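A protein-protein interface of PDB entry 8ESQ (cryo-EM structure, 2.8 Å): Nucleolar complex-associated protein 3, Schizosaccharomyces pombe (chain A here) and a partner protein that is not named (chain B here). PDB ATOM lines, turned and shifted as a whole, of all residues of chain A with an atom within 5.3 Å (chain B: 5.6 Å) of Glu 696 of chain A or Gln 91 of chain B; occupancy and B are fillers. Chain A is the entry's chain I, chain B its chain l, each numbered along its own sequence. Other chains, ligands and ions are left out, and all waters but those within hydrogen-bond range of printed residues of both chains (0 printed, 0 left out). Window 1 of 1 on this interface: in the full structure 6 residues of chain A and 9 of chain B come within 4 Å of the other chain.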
ATOM      1  N   TYR A 591     -38.411 -12.311  16.989  1.00  0.00           N
ATOM      2  CA  TYR A 591     -37.110 -12.128  17.620  1.00  0.00           C
ATOM      3  C   TYR A 591     -36.703 -10.660  17.655  1.00  0.00           C
ATOM      4  O   TYR A 591     -36.033 -10.223  18.597  1.00  0.00           O
ATOM      5  CB  TYR A 591     -36.067 -12.959  16.874  1.00  0.00           C
ATOM      6  CG  TYR A 591     -34.743 -13.110  17.583  1.00  0.00           C
ATOM      7  CD1 TYR A 591     -34.557 -14.104  18.530  1.00  0.00           C
ATOM      8  CD2 TYR A 591     -33.673 -12.278  17.289  1.00  0.00           C
ATOM      9  CE1 TYR A 591     -33.352 -14.261  19.177  1.00  0.00           C
ATOM     10  CE2 TYR A 591     -32.459 -12.427  17.932  1.00  0.00           C
ATOM     11  CZ  TYR A 591     -32.305 -13.423  18.872  1.00  0.00           C
ATOM     12  OH  TYR A 591     -31.103 -13.577  19.520  1.00  0.00           O
ATOM     13  N   SER A 649     -32.762 -26.195  21.244  1.00  0.00           N
ATOM     14  CA  SER A 649     -31.583 -26.666  20.520  1.00  0.00           C
ATOM     15  C   SER A 649     -30.497 -25.601  20.478  1.00  0.00           C
ATOM     16  O   SER A 649     -29.846 -25.410  19.446  1.00  0.00           O
ATOM     17  CB  SER A 649     -31.968 -27.098  19.109  1.00  0.00           C
ATOM     18  OG  SER A 649     -32.439 -25.997  18.349  1.00  0.00           O
ATOM     19  N   SER A 650     -30.312 -24.882  21.586  1.00  0.00           N
ATOM     20  CA  SER A 650     -29.438 -23.722  21.774  1.00  0.00           C
ATOM     21  C   SER A 650     -30.035 -22.479  21.124  1.00  0.00           C
ATOM     22  O   SER A 650     -29.441 -21.399  21.229  1.00  0.00           O
ATOM     23  CB  SER A 650     -28.009 -23.932  21.245  1.00  0.00           C
ATOM     24  OG  SER A 650     -27.353 -24.972  21.950  1.00  0.00           O
ATOM     25  N   ARG A 651     -31.183 -22.591  20.457  1.00  0.00           N
ATOM     26  CA  ARG A 651     -31.875 -21.432  19.913  1.00  0.00           C
ATOM     27  C   ARG A 651     -32.796 -20.772  20.928  1.00  0.00           C
ATOM     28  O   ARG A 651     -32.966 -19.546  20.896  1.00  0.00           O
ATOM     29  CB  ARG A 651     -32.675 -21.838  18.672  1.00  0.00           C
ATOM     30  CG  ARG A 651     -33.359 -20.686  17.963  1.00  0.00           C
ATOM     31  CD  ARG A 651     -32.381 -19.586  17.603  1.00  0.00           C
ATOM     32  NE  ARG A 651     -33.082 -18.385  17.169  1.00  0.00           N
ATOM     33  CZ  ARG A 651     -32.515 -17.198  17.009  1.00  0.00           C
ATOM     34  NH1 ARG A 651     -31.226 -17.009  17.239  1.00  0.00           N
ATOM     35  NH2 ARG A 651     -33.261 -16.174  16.606  1.00  0.00           N
ATOM     36  N   SER A 694     -23.415 -17.783  20.798  1.00  0.00           N
ATOM     37  CA  SER A 694     -23.507 -16.729  19.795  1.00  0.00           C
ATOM     38  C   SER A 694     -24.952 -16.312  19.564  1.00  0.00           C
ATOM     39  O   SER A 694     -25.825 -17.149  19.319  1.00  0.00           O
ATOM     40  CB  SER A 694     -22.883 -17.202  18.480  1.00  0.00           C
ATOM     41  OG  SER A 694     -21.519 -17.537  18.655  1.00  0.00           O
ATOM     42  N   GLU A 695     -25.198 -15.008  19.650  1.00  0.00           N
ATOM     43  CA  GLU A 695     -26.541 -14.461  19.489  1.00  0.00           C
ATOM     44  C   GLU A 695     -26.734 -14.013  18.041  1.00  0.00           C
ATOM     45  O   GLU A 695     -26.795 -12.829  17.715  1.00  0.00           O
ATOM     46  CB  GLU A 695     -26.767 -13.321  20.478  1.00  0.00           C
ATOM     47  CG  GLU A 695     -28.216 -12.890  20.613  1.00  0.00           C
ATOM     48  CD  GLU A 695     -28.514 -11.613  19.859  1.00  0.00           C
ATOM     49  OE1 GLU A 695     -27.579 -10.811  19.658  1.00  0.00           O
ATOM     50  OE2 GLU A 695     -29.681 -11.412  19.462  1.00  0.00           O
ATOM     51  N   GLU A 696     -26.838 -15.010  17.166  1.00  0.00           N
ATOM     52  CA  GLU A 696     -27.037 -14.781  15.741  1.00  0.00           C
ATOM     53  C   GLU A 696     -28.487 -14.405  15.463  1.00  0.00           C
ATOM     54  O   GLU A 696     -29.227 -14.063  16.392  1.00  0.00           O
ATOM     55  CB  GLU A 696     -26.634 -16.025  14.949  1.00  0.00           C
ATOM     56  CG  GLU A 696     -27.271 -17.303  15.462  1.00  0.00           C
ATOM     57  CD  GLU A 696     -26.853 -18.525  14.672  1.00  0.00           C
ATOM     58  OE1 GLU A 696     -26.041 -18.380  13.735  1.00  0.00           O
ATOM     59  OE2 GLU A 696     -27.337 -19.632  14.990  1.00  0.00           O
ATOM     60  N   GLN A 697     -28.902 -14.459  14.196  1.00  0.00           N
ATOM     61  CA  GLN A 697     -30.267 -14.104  13.801  1.00  0.00           C
ATOM     62  C   GLN A 697     -30.594 -12.658  14.182  1.00  0.00           C
ATOM     63  O   GLN A 697     -31.358 -12.392  15.112  1.00  0.00           O
ATOM     64  CB  GLN A 697     -31.288 -15.081  14.395  1.00  0.00           C
ATOM     65  CG  GLN A 697     -31.443 -16.384  13.623  1.00  0.00           C
ATOM     66  CD  GLN A 697     -30.352 -17.389  13.932  1.00  0.00           C
ATOM     67  OE1 GLN A 697     -30.371 -18.042  14.976  1.00  0.00           O
ATOM     68  NE2 GLN A 697     -29.403 -17.530  13.016  1.00  0.00           N
ATOM     69  N   ILE A 698     -29.932 -11.732  13.473  1.00  0.00           N
ATOM     70  CA  ILE A 698     -30.111 -10.276  13.510  1.00  0.00           C
ATOM     71  C   ILE A 698     -29.158  -9.676  14.540  1.00  0.00           C
ATOM     72  O   ILE A 698     -28.946  -8.458  14.572  1.00  0.00           O
ATOM     73  CB  ILE A 698     -31.573  -9.851  13.786  1.00  0.00           C
ATOM     74  CG1 ILE A 698     -32.548 -10.544  12.831  1.00  0.00           C
ATOM     75  CG2 ILE A 698     -31.760  -8.347  13.628  1.00  0.00           C
ATOM     76  CD1 ILE A 698     -33.985 -10.413  13.265  1.00  0.00           C
ATOM     77  N   GLY A 699     -28.525 -10.530  15.342  1.00  0.00           N
ATOM     78  CA  GLY A 699     -27.547 -10.077  16.312  1.00  0.00           C
ATOM     79  C   GLY A 699     -28.017  -8.952  17.213  1.00  0.00           C
ATOM     80  O   GLY A 699     -29.007  -9.101  17.934  1.00  0.00           O
ATOM     81  N   TYR A 703     -22.613 -11.586  21.529  1.00  0.00           N
ATOM     82  CA  TYR A 703     -22.545 -12.942  20.997  1.00  0.00           C
ATOM     83  C   TYR A 703     -21.872 -13.888  21.983  1.00  0.00           C
ATOM     84  O   TYR A 703     -22.430 -14.936  22.326  1.00  0.00           O
ATOM     85  CB  TYR A 703     -21.797 -12.952  19.662  1.00  0.00           C
ATOM     86  CG  TYR A 703     -22.662 -12.672  18.456  1.00  0.00           C
ATOM     87  CD1 TYR A 703     -23.406 -11.502  18.363  1.00  0.00           C
ATOM     88  CD2 TYR A 703     -22.740 -13.582  17.409  1.00  0.00           C
ATOM     89  CE1 TYR A 703     -24.196 -11.244  17.258  1.00  0.00           C
ATOM     90  CE2 TYR A 703     -23.529 -13.334  16.302  1.00  0.00           C
ATOM     91  CZ  TYR A 703     -24.254 -12.165  16.231  1.00  0.00           C
ATOM     92  OH  TYR A 703     -25.041 -11.917  15.130  1.00  0.00           O
ATOM     93  N   HIS B  26     -28.449 -17.715   6.557  1.00  0.00           N
ATOM     94  CA  HIS B  26     -27.644 -17.123   7.622  1.00  0.00           C
ATOM     95  C   HIS B  26     -26.149 -17.320   7.371  1.00  0.00           C
ATOM     96  O   HIS B  26     -25.314 -16.588   7.916  1.00  0.00           O
ATOM     97  CB  HIS B  26     -28.072 -17.675   8.986  1.00  0.00           C
ATOM     98  CG  HIS B  26     -29.543 -17.951   9.105  1.00  0.00           C
ATOM     99  ND1 HIS B  26     -30.047 -19.131   9.610  1.00  0.00           N
ATOM    100  CD2 HIS B  26     -30.618 -17.177   8.820  1.00  0.00           C
ATOM    101  CE1 HIS B  26     -31.367 -19.077   9.620  1.00  0.00           C
ATOM    102  NE2 HIS B  26     -31.740 -17.903   9.140  1.00  0.00           N
ATOM    103  N   LEU B  86     -19.134 -30.056  10.418  1.00  0.00           N
ATOM    104  CA  LEU B  86     -20.160 -30.692  11.237  1.00  0.00           C
ATOM    105  C   LEU B  86     -20.805 -29.718  12.212  1.00  0.00           C
ATOM    106  O   LEU B  86     -22.018 -29.783  12.440  1.00  0.00           O
ATOM    107  CB  LEU B  86     -19.562 -31.873  11.999  1.00  0.00           C
ATOM    108  CG  LEU B  86     -20.485 -32.556  13.006  1.00  0.00           C
ATOM    109  CD1 LEU B  86     -21.708 -33.125  12.305  1.00  0.00           C
ATOM    110  CD2 LEU B  86     -19.735 -33.641  13.755  1.00  0.00           C
ATOM    111  N   ASP B  87     -20.019 -28.810  12.795  1.00  0.00           N
ATOM    112  CA  ASP B  87     -20.581 -27.849  13.740  1.00  0.00           C
ATOM    113  C   ASP B  87     -21.606 -26.948  13.061  1.00  0.00           C
ATOM    114  O   ASP B  87     -22.691 -26.702  13.601  1.00  0.00           O
ATOM    115  CB  ASP B  87     -19.464 -27.016  14.370  1.00  0.00           C
ATOM    116  CG  ASP B  87     -18.516 -26.431  13.339  1.00  0.00           C
ATOM    117  OD1 ASP B  87     -17.835 -27.213  12.642  1.00  0.00           O
ATOM    118  OD2 ASP B  87     -18.456 -25.189  13.225  1.00  0.00           O
ATOM    119  N   TYR B  88     -21.279 -26.448  11.867  1.00  0.00           N
ATOM    120  CA  TYR B  88     -22.222 -25.607  11.137  1.00  0.00           C
ATOM    121  C   TYR B  88     -23.429 -26.406  10.665  1.00  0.00           C
ATOM    122  O   TYR B  88     -24.569 -25.938  10.768  1.00  0.00           O
ATOM    123  CB  TYR B  88     -21.520 -24.941   9.957  1.00  0.00           C
ATOM    124  CG  TYR B  88     -20.758 -23.697  10.341  1.00  0.00           C
ATOM    125  CD1 TYR B  88     -20.868 -23.159  11.617  1.00  0.00           C
ATOM    126  CD2 TYR B  88     -19.917 -23.068   9.437  1.00  0.00           C
ATOM    127  CE1 TYR B  88     -20.172 -22.021  11.976  1.00  0.00           C
ATOM    128  CE2 TYR B  88     -19.216 -21.935   9.790  1.00  0.00           C
ATOM    129  CZ  TYR B  88     -19.345 -21.414  11.056  1.00  0.00           C
ATOM    130  OH  TYR B  88     -18.646 -20.282  11.401  1.00  0.00           O
ATOM    131  N   ILE B  89     -23.201 -27.613  10.146  1.00  0.00           N
ATOM    132  CA  ILE B  89     -24.306 -28.433   9.658  1.00  0.00           C
ATOM    133  C   ILE B  89     -25.226 -28.831  10.806  1.00  0.00           C
ATOM    134  O   ILE B  89     -26.454 -28.832  10.662  1.00  0.00           O
ATOM    135  CB  ILE B  89     -23.769 -29.658   8.889  1.00  0.00           C
ATOM    136  CG1 ILE B  89     -23.481 -29.317   7.419  1.00  0.00           C
ATOM    137  CG2 ILE B  89     -24.728 -30.827   8.979  1.00  0.00           C
ATOM    138  CD1 ILE B  89     -22.528 -28.170   7.178  1.00  0.00           C
ATOM    139  N   ALA B  90     -24.652 -29.153  11.967  1.00  0.00           N
ATOM    140  CA  ALA B  90     -25.477 -29.527  13.113  1.00  0.00           C
ATOM    141  C   ALA B  90     -26.308 -28.352  13.617  1.00  0.00           C
ATOM    142  O   ALA B  90     -27.483 -28.521  13.961  1.00  0.00           O
ATOM    143  CB  ALA B  90     -24.602 -30.076  14.236  1.00  0.00           C
ATOM    144  N   GLN B  91     -25.713 -27.159  13.688  1.00  0.00           N
ATOM    145  CA  GLN B  91     -26.445 -26.006  14.201  1.00  0.00           C
ATOM    146  C   GLN B  91     -27.640 -25.689  13.309  1.00  0.00           C
ATOM    147  O   GLN B  91     -28.778 -25.658  13.792  1.00  0.00           O
ATOM    148  CB  GLN B  91     -25.471 -24.823  14.332  1.00  0.00           C
ATOM    149  CG  GLN B  91     -25.961 -23.354  14.462  1.00  0.00           C
ATOM    150  CD  GLN B  91     -27.270 -23.131  15.203  1.00  0.00           C
ATOM    151  OE1 GLN B  91     -28.354 -23.277  14.647  1.00  0.00           O
ATOM    152  NE2 GLN B  91     -27.167 -22.778  16.477  1.00  0.00           N
ATOM    153  N   TYR B  92     -27.420 -25.583  12.001  1.00  0.00           N
ATOM    154  CA  TYR B  92     -28.451 -25.186  11.050  1.00  0.00           C
ATOM    155  C   TYR B  92     -29.182 -26.409  10.504  1.00  0.00           C
ATOM    156  O   TYR B  92     -29.833 -26.342   9.459  1.00  0.00           O
ATOM    157  CB  TYR B  92     -27.839 -24.379   9.904  1.00  0.00           C
ATOM    158  CG  TYR B  92     -27.097 -23.118  10.310  1.00  0.00           C
ATOM    159  CD1 TYR B  92     -25.882 -23.188  10.979  1.00  0.00           C
ATOM    160  CD2 TYR B  92     -27.592 -21.861   9.991  1.00  0.00           C
ATOM    161  CE1 TYR B  92     -25.195 -22.046  11.341  1.00  0.00           C
ATOM    162  CE2 TYR B  92     -26.912 -20.711  10.349  1.00  0.00           C
ATOM    163  CZ  TYR B  92     -25.715 -20.810  11.024  1.00  0.00           C
ATOM    164  OH  TYR B  92     -25.033 -19.670  11.383  1.00  0.00           O
ATOM    165  N   ALA B  93     -29.094 -27.530  11.218  1.00  0.00           N
ATOM    166  CA  ALA B  93     -29.665 -28.784  10.749  1.00  0.00           C
ATOM    167  C   ALA B  93     -31.181 -28.709  10.742  1.00  0.00           C
ATOM    168  O   ALA B  93     -31.802 -28.391  11.761  1.00  0.00           O
ATOM    169  CB  ALA B  93     -29.210 -29.944  11.634  1.00  0.00           C
ATOM    170  N   TYR B 134     -26.895 -37.117  16.213  1.00  0.00           N
ATOM    171  CA  TYR B 134     -26.635 -36.517  17.513  1.00  0.00           C
ATOM    172  C   TYR B 134     -26.540 -37.615  18.565  1.00  0.00           C
ATOM    173  O   TYR B 134     -27.087 -38.707  18.399  1.00  0.00           O
ATOM    174  CB  TYR B 134     -27.747 -35.532  17.912  1.00  0.00           C
ATOM    175  CG  TYR B 134     -27.639 -34.140  17.326  1.00  0.00           C
ATOM    176  CD1 TYR B 134     -27.330 -33.946  15.985  1.00  0.00           C
ATOM    177  CD2 TYR B 134     -27.875 -33.021  18.111  1.00  0.00           C
ATOM    178  CE1 TYR B 134     -27.244 -32.672  15.449  1.00  0.00           C
ATOM    179  CE2 TYR B 134     -27.794 -31.748  17.583  1.00  0.00           C
ATOM    180  CZ  TYR B 134     -27.476 -31.578  16.255  1.00  0.00           C
ATOM    181  OH  TYR B 134     -27.399 -30.305  15.738  1.00  0.00           O
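The side-chain carboxylate (OE2) of Glu 696 of chain A sits at hydrogen-bond distance from the side-chain amide nitrogen (NE2) of Gln 91 of chain B, 3.5 Å away. The side-chain carboxylate (OE1) of Glu 696 of chain A lies within hydrogen-bond range of the side-chain hydroxyl (OH) of Tyr 92 of chain B, 2.9 Å away.
NH1 of Arg 651 of chain A sits at hydrogen-bond distance from OE1 of Gln 697 of chain A. The side-chain carboxylate (OE2) of Glu 696 of chain A sits close to the side-chain amide oxygen (OE1) of Gln 697 of chain A, at 3.4 Å.
Among the printed residues, pairs that only touch across the chains: Gln 697 of chain A with His 26 of chain B (3.8 Å).
Ser 649 of chain A touches none of the printed residues of chain B. Of the printed residues of chain B, Glu 696 of chain A touches Gln 91 and Tyr 92. Of the printed residues of chain B, Gln 697 of chain A touches His 26 (3.8 Å). Tyr 703 of chain A touches none of the printed residues of chain B. Of the printed residues of chain A, His 26 of chain B touches Gln 697 (3.8 Å). Gln 91 of chain B touches one residue of chain A. Of the printed residues of chain A, Tyr 92 of chain B touches Glu 696. The nearest residue of chain B that does not touch Glu 696 of chain A is His 26 of chain B (5.2 Å). The nearest residue of chain A that does not touch Gln 91 of chain B is Ser 649 of chain A (4.8 Å).
Hydrophobic or aromatic side chains of chain B within 4 Å of the printed part of chain A: His 26 and Tyr 92. Among the printed residues, 3 pairs touch across the chains. Among the printed residues, no Asp or Glu carboxylate lies within 4 Å of a Lys or Arg side-chain nitrogen of the other chain.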
